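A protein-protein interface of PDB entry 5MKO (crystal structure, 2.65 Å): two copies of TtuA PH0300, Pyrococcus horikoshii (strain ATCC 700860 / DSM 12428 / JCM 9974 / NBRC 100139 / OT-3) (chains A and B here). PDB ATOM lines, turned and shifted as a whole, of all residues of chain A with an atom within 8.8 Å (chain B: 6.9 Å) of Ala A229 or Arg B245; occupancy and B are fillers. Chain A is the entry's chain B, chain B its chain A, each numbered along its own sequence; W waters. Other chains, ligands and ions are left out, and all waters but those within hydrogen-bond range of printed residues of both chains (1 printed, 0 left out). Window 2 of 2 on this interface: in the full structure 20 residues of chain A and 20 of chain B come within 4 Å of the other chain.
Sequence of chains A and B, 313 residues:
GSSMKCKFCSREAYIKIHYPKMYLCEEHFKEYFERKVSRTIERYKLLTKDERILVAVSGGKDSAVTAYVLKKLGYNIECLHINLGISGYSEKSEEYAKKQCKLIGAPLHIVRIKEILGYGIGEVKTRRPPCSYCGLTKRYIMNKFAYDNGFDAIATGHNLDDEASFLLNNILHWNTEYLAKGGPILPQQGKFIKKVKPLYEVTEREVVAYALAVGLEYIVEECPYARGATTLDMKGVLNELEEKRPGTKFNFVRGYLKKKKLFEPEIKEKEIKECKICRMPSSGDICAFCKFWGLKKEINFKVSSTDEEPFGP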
ATOM      1  N   ASN A 169      17.473  28.089   1.894  1.00  0.00           N
ATOM      2  CA  ASN A 169      16.810  29.082   2.724  1.00  0.00           C
ATOM      3  C   ASN A 169      17.530  30.431   2.730  1.00  0.00           C
ATOM      4  O   ASN A 169      16.867  31.468   2.674  1.00  0.00           O
ATOM      5  CB  ASN A 169      16.575  28.557   4.142  1.00  0.00           C
ATOM      6  CG  ASN A 169      15.704  29.462   4.974  1.00  0.00           C
ATOM      7  OD1 ASN A 169      14.679  29.981   4.519  1.00  0.00           O
ATOM      8  ND2 ASN A 169      16.110  29.696   6.206  1.00  0.00           N
ATOM      9  N   LEU A 172      17.240  32.165  -0.824  1.00  0.00           N
ATOM     10  CA  LEU A 172      15.909  32.765  -0.928  1.00  0.00           C
ATOM     11  C   LEU A 172      15.802  34.090  -0.167  1.00  0.00           C
ATOM     12  O   LEU A 172      15.115  34.999  -0.633  1.00  0.00           O
ATOM     13  CB  LEU A 172      14.834  31.785  -0.431  1.00  0.00           C
ATOM     14  CG  LEU A 172      14.450  30.631  -1.355  1.00  0.00           C
ATOM     15  CD1 LEU A 172      13.626  29.615  -0.606  1.00  0.00           C
ATOM     16  CD2 LEU A 172      13.678  31.116  -2.577  1.00  0.00           C
ATOM     17  N   HIS A 173      16.481  34.195   0.991  1.00  0.00           N
ATOM     18  CA  HIS A 173      16.511  35.394   1.835  1.00  0.00           C
ATOM     19  C   HIS A 173      17.706  36.287   1.544  1.00  0.00           C
ATOM     20  O   HIS A 173      17.779  37.397   2.078  1.00  0.00           O
ATOM     21  CB  HIS A 173      16.512  35.007   3.314  1.00  0.00           C
ATOM     22  CG  HIS A 173      15.194  34.486   3.778  1.00  0.00           C
ATOM     23  ND1 HIS A 173      15.035  33.171   4.157  1.00  0.00           N
ATOM     24  CD2 HIS A 173      14.002  35.116   3.871  1.00  0.00           C
ATOM     25  CE1 HIS A 173      13.761  33.047   4.486  1.00  0.00           C
ATOM     26  NE2 HIS A 173      13.101  34.190   4.327  1.00  0.00           N
ATOM     27  N   GLY A 228       6.785  26.671  13.465  1.00  0.00           N
ATOM     28  CA  GLY A 228       7.141  26.816  12.057  1.00  0.00           C
ATOM     29  C   GLY A 228       8.059  25.723  11.553  1.00  0.00           C
ATOM     30  O   GLY A 228       9.008  25.342  12.248  1.00  0.00           O
ATOM     31  N   ALA A 229       7.785  25.211  10.333  1.00  0.00           N
ATOM     32  CA  ALA A 229       8.578  24.144   9.717  1.00  0.00           C
ATOM     33  C   ALA A 229       9.284  24.615   8.434  1.00  0.00           C
ATOM     34  O   ALA A 229       9.068  24.039   7.365  1.00  0.00           O
ATOM     35  CB  ALA A 229       7.701  22.921   9.448  1.00  0.00           C
ATOM     36  N   THR A 230      10.143  25.656   8.558  1.00  0.00           N
ATOM     37  CA  THR A 230      10.914  26.247   7.452  1.00  0.00           C
ATOM     38  C   THR A 230      11.864  25.229   6.811  1.00  0.00           C
ATOM     39  O   THR A 230      11.848  25.081   5.589  1.00  0.00           O
ATOM     40  CB  THR A 230      11.624  27.536   7.904  1.00  0.00           C
ATOM     41  OG1 THR A 230      10.654  28.430   8.455  1.00  0.00           O
ATOM     42  CG2 THR A 230      12.376  28.226   6.767  1.00  0.00           C
ATOM     43  N   THR A 231      12.667  24.525   7.635  1.00  0.00           N
ATOM     44  CA  THR A 231      13.624  23.510   7.181  1.00  0.00           C
ATOM     45  C   THR A 231      12.927  22.351   6.465  1.00  0.00           C
ATOM     46  O   THR A 231      13.389  21.952   5.397  1.00  0.00           O
ATOM     47  CB  THR A 231      14.539  23.042   8.319  1.00  0.00           C
ATOM     48  OG1 THR A 231      13.741  22.539   9.389  1.00  0.00           O
ATOM     49  CG2 THR A 231      15.468  24.145   8.818  1.00  0.00           C
ATOM     50  N   LEU A 232      11.799  21.847   7.022  1.00  0.00           N
ATOM     51  CA  LEU A 232      11.012  20.762   6.421  1.00  0.00           C
ATOM     52  C   LEU A 232      10.427  21.145   5.066  1.00  0.00           C
ATOM     53  O   LEU A 232      10.336  20.293   4.181  1.00  0.00           O
ATOM     54  CB  LEU A 232       9.914  20.268   7.368  1.00  0.00           C
ATOM     55  CG  LEU A 232      10.346  19.243   8.408  1.00  0.00           C
ATOM     56  CD1 LEU A 232       9.317  19.146   9.516  1.00  0.00           C
ATOM     57  CD2 LEU A 232      10.573  17.863   7.777  1.00  0.00           C
ATOM     58  N   ASP A 233      10.057  22.433   4.906  1.00  0.00           N
ATOM     59  CA  ASP A 233       9.547  23.001   3.662  1.00  0.00           C
ATOM     60  C   ASP A 233      10.660  22.980   2.610  1.00  0.00           C
ATOM     61  O   ASP A 233      10.411  22.535   1.488  1.00  0.00           O
ATOM     62  CB  ASP A 233       9.028  24.438   3.878  1.00  0.00           C
ATOM     63  CG  ASP A 233       7.704  24.564   4.625  1.00  0.00           C
ATOM     64  OD1 ASP A 233       7.048  23.520   4.866  1.00  0.00           O
ATOM     65  OD2 ASP A 233       7.330  25.707   4.979  1.00  0.00           O
ATOM     66  N   MET A 234      11.895  23.407   2.989  1.00  0.00           N
ATOM     67  CA  MET A 234      13.058  23.420   2.093  1.00  0.00           C
ATOM     68  C   MET A 234      13.462  21.996   1.729  1.00  0.00           C
ATOM     69  O   MET A 234      13.766  21.726   0.566  1.00  0.00           O
ATOM     70  CB  MET A 234      14.264  24.149   2.714  1.00  0.00           C
ATOM     71  CG  MET A 234      14.010  25.576   3.106  1.00  0.00           C
ATOM     72  SD  MET A 234      13.531  26.663   1.751  1.00  0.00           S
ATOM     73  CE  MET A 234      12.755  27.976   2.680  1.00  0.00           C
ATOM     74  N   LYS A 235      13.438  21.085   2.726  1.00  0.00           N
ATOM     75  CA  LYS A 235      13.785  19.676   2.562  1.00  0.00           C
ATOM     76  C   LYS A 235      12.839  18.951   1.610  1.00  0.00           C
ATOM     77  O   LYS A 235      13.317  18.269   0.704  1.00  0.00           O
ATOM     78  CB  LYS A 235      13.896  18.965   3.916  1.00  0.00           C
ATOM     79  CG  LYS A 235      15.234  19.227   4.580  1.00  0.00           C
ATOM     80  CD  LYS A 235      15.318  18.639   5.960  1.00  0.00           C
ATOM     81  CE  LYS A 235      16.734  18.660   6.461  1.00  0.00           C
ATOM     82  NZ  LYS A 235      16.828  18.083   7.825  1.00  0.00           N
ATOM     83  N   GLY A 236      11.530  19.153   1.783  1.00  0.00           N
ATOM     84  CA  GLY A 236      10.511  18.565   0.924  1.00  0.00           C
ATOM     85  C   GLY A 236      10.651  19.008  -0.519  1.00  0.00           C
ATOM     86  O   GLY A 236      10.558  18.192  -1.441  1.00  0.00           O
ATOM     87  N   LEU B 238       8.584  26.700  -6.460  1.00  0.00           N
ATOM     88  CA  LEU B 238       8.473  28.068  -5.953  1.00  0.00           C
ATOM     89  C   LEU B 238       7.033  28.432  -5.600  1.00  0.00           C
ATOM     90  O   LEU B 238       6.825  29.248  -4.703  1.00  0.00           O
ATOM     91  CB  LEU B 238       9.078  29.076  -6.940  1.00  0.00           C
ATOM     92  CG  LEU B 238      10.595  29.047  -7.099  1.00  0.00           C
ATOM     93  CD1 LEU B 238      10.987  29.432  -8.488  1.00  0.00           C
ATOM     94  CD2 LEU B 238      11.273  29.962  -6.114  1.00  0.00           C
ATOM     95  N   GLU B 240       4.864  26.144  -4.397  1.00  0.00           N
ATOM     96  CA  GLU B 240       4.686  25.410  -3.143  1.00  0.00           C
ATOM     97  C   GLU B 240       5.190  26.299  -1.986  1.00  0.00           C
ATOM     98  O   GLU B 240       4.454  26.518  -1.021  1.00  0.00           O
ATOM     99  CB  GLU B 240       5.475  24.092  -3.184  1.00  0.00           C
ATOM    100  CG  GLU B 240       4.932  23.009  -2.266  1.00  0.00           C
ATOM    101  CD  GLU B 240       5.916  21.888  -1.982  1.00  0.00           C
ATOM    102  OE1 GLU B 240       5.990  20.934  -2.791  1.00  0.00           O
ATOM    103  OE2 GLU B 240       6.634  21.978  -0.960  1.00  0.00           O
ATOM    104  N   LEU B 241       6.414  26.866  -2.136  1.00  0.00           N
ATOM    105  CA  LEU B 241       7.047  27.770  -1.172  1.00  0.00           C
ATOM    106  C   LEU B 241       6.231  29.032  -0.961  1.00  0.00           C
ATOM    107  O   LEU B 241       6.100  29.472   0.180  1.00  0.00           O
ATOM    108  CB  LEU B 241       8.478  28.151  -1.602  1.00  0.00           C
ATOM    109  CG  LEU B 241       9.533  27.040  -1.678  1.00  0.00           C
ATOM    110  CD1 LEU B 241      10.829  27.582  -2.241  1.00  0.00           C
ATOM    111  CD2 LEU B 241       9.799  26.410  -0.314  1.00  0.00           C
ATOM    112  N   GLU B 242       5.687  29.610  -2.058  1.00  0.00           N
ATOM    113  CA  GLU B 242       4.865  30.826  -2.053  1.00  0.00           C
ATOM    114  C   GLU B 242       3.557  30.598  -1.294  1.00  0.00           C
ATOM    115  O   GLU B 242       3.113  31.490  -0.571  1.00  0.00           O
ATOM    116  CB  GLU B 242       4.579  31.295  -3.491  1.00  0.00           C
ATOM    117  CG  GLU B 242       3.998  32.700  -3.614  1.00  0.00           C
ATOM    118  CD  GLU B 242       4.935  33.874  -3.389  1.00  0.00           C
ATOM    119  OE1 GLU B 242       6.170  33.693  -3.483  1.00  0.00           O
ATOM    120  OE2 GLU B 242       4.425  34.995  -3.163  1.00  0.00           O
ATOM    121  N   GLU B 243       2.953  29.398  -1.459  1.00  0.00           N
ATOM    122  CA  GLU B 243       1.698  28.981  -0.815  1.00  0.00           C
ATOM    123  C   GLU B 243       1.822  28.994   0.722  1.00  0.00           C
ATOM    124  O   GLU B 243       0.873  29.365   1.413  1.00  0.00           O
ATOM    125  CB  GLU B 243       1.297  27.584  -1.318  1.00  0.00           C
ATOM    126  CG  GLU B 243      -0.159  27.215  -1.088  1.00  0.00           C
ATOM    127  CD  GLU B 243      -0.654  26.019  -1.881  1.00  0.00           C
ATOM    128  OE1 GLU B 243       0.094  25.019  -2.003  1.00  0.00           O
ATOM    129  OE2 GLU B 243      -1.812  26.073  -2.356  1.00  0.00           O
ATOM    130  N   LYS B 244       2.993  28.602   1.241  1.00  0.00           N
ATOM    131  CA  LYS B 244       3.279  28.572   2.671  1.00  0.00           C
ATOM    132  C   LYS B 244       3.703  29.964   3.155  1.00  0.00           C
ATOM    133  O   LYS B 244       3.156  30.454   4.146  1.00  0.00           O
ATOM    134  CB  LYS B 244       4.357  27.518   2.988  1.00  0.00           C
ATOM    135  CG  LYS B 244       3.894  26.082   2.786  1.00  0.00           C
ATOM    136  CD  LYS B 244       5.021  25.213   2.268  1.00  0.00           C
ATOM    137  CE  LYS B 244       4.581  23.785   2.050  1.00  0.00           C
ATOM    138  NZ  LYS B 244       5.698  22.924   1.572  1.00  0.00           N
ATOM    139  N   ARG B 245       4.673  30.597   2.451  1.00  0.00           N
ATOM    140  CA  ARG B 245       5.200  31.922   2.782  1.00  0.00           C
ATOM    141  C   ARG B 245       4.970  32.892   1.609  1.00  0.00           C
ATOM    142  O   ARG B 245       5.734  32.864   0.645  1.00  0.00           O
ATOM    143  CB  ARG B 245       6.699  31.868   3.160  1.00  0.00           C
ATOM    144  CG  ARG B 245       7.152  30.624   3.922  1.00  0.00           C
ATOM    145  CD  ARG B 245       7.205  30.814   5.433  1.00  0.00           C
ATOM    146  NE  ARG B 245       7.819  29.661   6.102  1.00  0.00           N
ATOM    147  CZ  ARG B 245       7.146  28.627   6.600  1.00  0.00           C
ATOM    148  NH1 ARG B 245       5.821  28.586   6.519  1.00  0.00           N
ATOM    149  NH2 ARG B 245       7.790  27.626   7.184  1.00  0.00           N
ATOM    150  N   PRO B 246       3.912  33.734   1.637  1.00  0.00           N
ATOM    151  CA  PRO B 246       3.683  34.656   0.507  1.00  0.00           C
ATOM    152  C   PRO B 246       4.736  35.758   0.458  1.00  0.00           C
ATOM    153  O   PRO B 246       5.201  36.214   1.503  1.00  0.00           O
ATOM    154  CB  PRO B 246       2.272  35.197   0.769  1.00  0.00           C
ATOM    155  CG  PRO B 246       1.681  34.281   1.827  1.00  0.00           C
ATOM    156  CD  PRO B 246       2.864  33.894   2.659  1.00  0.00           C
ATOM    157  N   GLY B 247       5.140  36.128  -0.752  1.00  0.00           N
ATOM    158  CA  GLY B 247       6.191  37.112  -0.981  1.00  0.00           C
ATOM    159  C   GLY B 247       7.567  36.495  -1.176  1.00  0.00           C
ATOM    160  O   GLY B 247       8.543  37.228  -1.338  1.00  0.00           O
ATOM    161  N   THR B 248       7.657  35.137  -1.165  1.00  0.00           N
ATOM    162  CA  THR B 248       8.896  34.369  -1.376  1.00  0.00           C
ATOM    163  C   THR B 248       9.547  34.749  -2.714  1.00  0.00           C
ATOM    164  O   THR B 248      10.696  35.192  -2.717  1.00  0.00           O
ATOM    165  CB  THR B 248       8.646  32.839  -1.226  1.00  0.00           C
ATOM    166  OG1 THR B 248       8.227  32.574   0.103  1.00  0.00           O
ATOM    167  CG2 THR B 248       9.899  31.989  -1.513  1.00  0.00           C
ATOM    168  N   LYS B 249       8.792  34.605  -3.832  1.00  0.00           N
ATOM    169  CA  LYS B 249       9.230  34.910  -5.197  1.00  0.00           C
ATOM    170  C   LYS B 249       9.713  36.347  -5.303  1.00  0.00           C
ATOM    171  O   LYS B 249      10.780  36.594  -5.871  1.00  0.00           O
ATOM    172  CB  LYS B 249       8.094  34.680  -6.200  1.00  0.00           C
ATOM    173  CG  LYS B 249       7.710  33.232  -6.435  1.00  0.00           C
ATOM    174  CD  LYS B 249       6.518  33.180  -7.358  1.00  0.00           C
ATOM    175  CE  LYS B 249       5.643  31.991  -7.079  1.00  0.00           C
ATOM    176  NZ  LYS B 249       4.300  32.140  -7.702  1.00  0.00           N
HETATM  177  O   HOH W   1       8.127  21.073   1.202  1.00  0.00           O
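The side-chain carboxylate of Asp A233 is in salt-bridge range of the side-chain amino group of Lys B244. The guanidinium group of Arg B245 is in salt-bridge range of the side-chain carboxylate of Asp A233 (3.0 Å). The guanidinium group of Arg B245 lies within hydrogen-bond range of the side-chain hydroxyl of Thr A230, 3.2 Å away.
OE2 of Glu B240 lies within salt-bridge range of NZ of Lys B244, at 2.9 Å. OG1 of Thr B248 is in hydrogen-bond range of O of Arg B245 (2.6 Å).
Among the printed residues, merely in contact across the chains: Leu A172 with Leu B241 and Ala A229 with Arg B245.
Ala A229 touches just one residue of chain B: Arg B245. Of chain A, only Ala A229, Thr A230 and Asp A233 come within 4 Å of Arg B245. Pro B246 touches none of the printed residues of chain A. Printed residues of chain B within 4 Å of Thr A230: Arg B245. Of the printed residues of chain B, Leu A172 touches Leu B241 (3.8 Å). Printed residues of chain A within 4 Å of Leu B241: Leu A172. Gly B247 touches none of the printed residues of chain A. The nearest residue of chain B that does not touch Ala A229 is Lys B244 (6.6 Å).
Of the 11 printed residues of chain B, 3 touch a printed residue of chain A. Printed residues of chain B that touch a printed residue of chain A: Leu B241, Lys B244 and Arg B245. Hydrophobic or aromatic side chains of chain B within 4 Å of the printed part of chain A: Leu B241. Of the 12 printed residues of chain A, 4 touch a printed residue of chain B. Among the printed residues, Asp or Glu carboxylates within 4 Å of a Lys or Arg side-chain nitrogen of the other chain: Asp A233 with Lys B244 and Asp A233 with Arg B245.
No position is printed for both chains. Of the 5 pairs that touch across the chains among the printed residues, none has its exchanged pair printed and touching as well.
Water W1 lies within hydrogen-bond range of the backbone carbonyl oxygen of Asp A233, the side-chain carboxylate of Glu B240 and the side-chain amino group of Lys B244.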
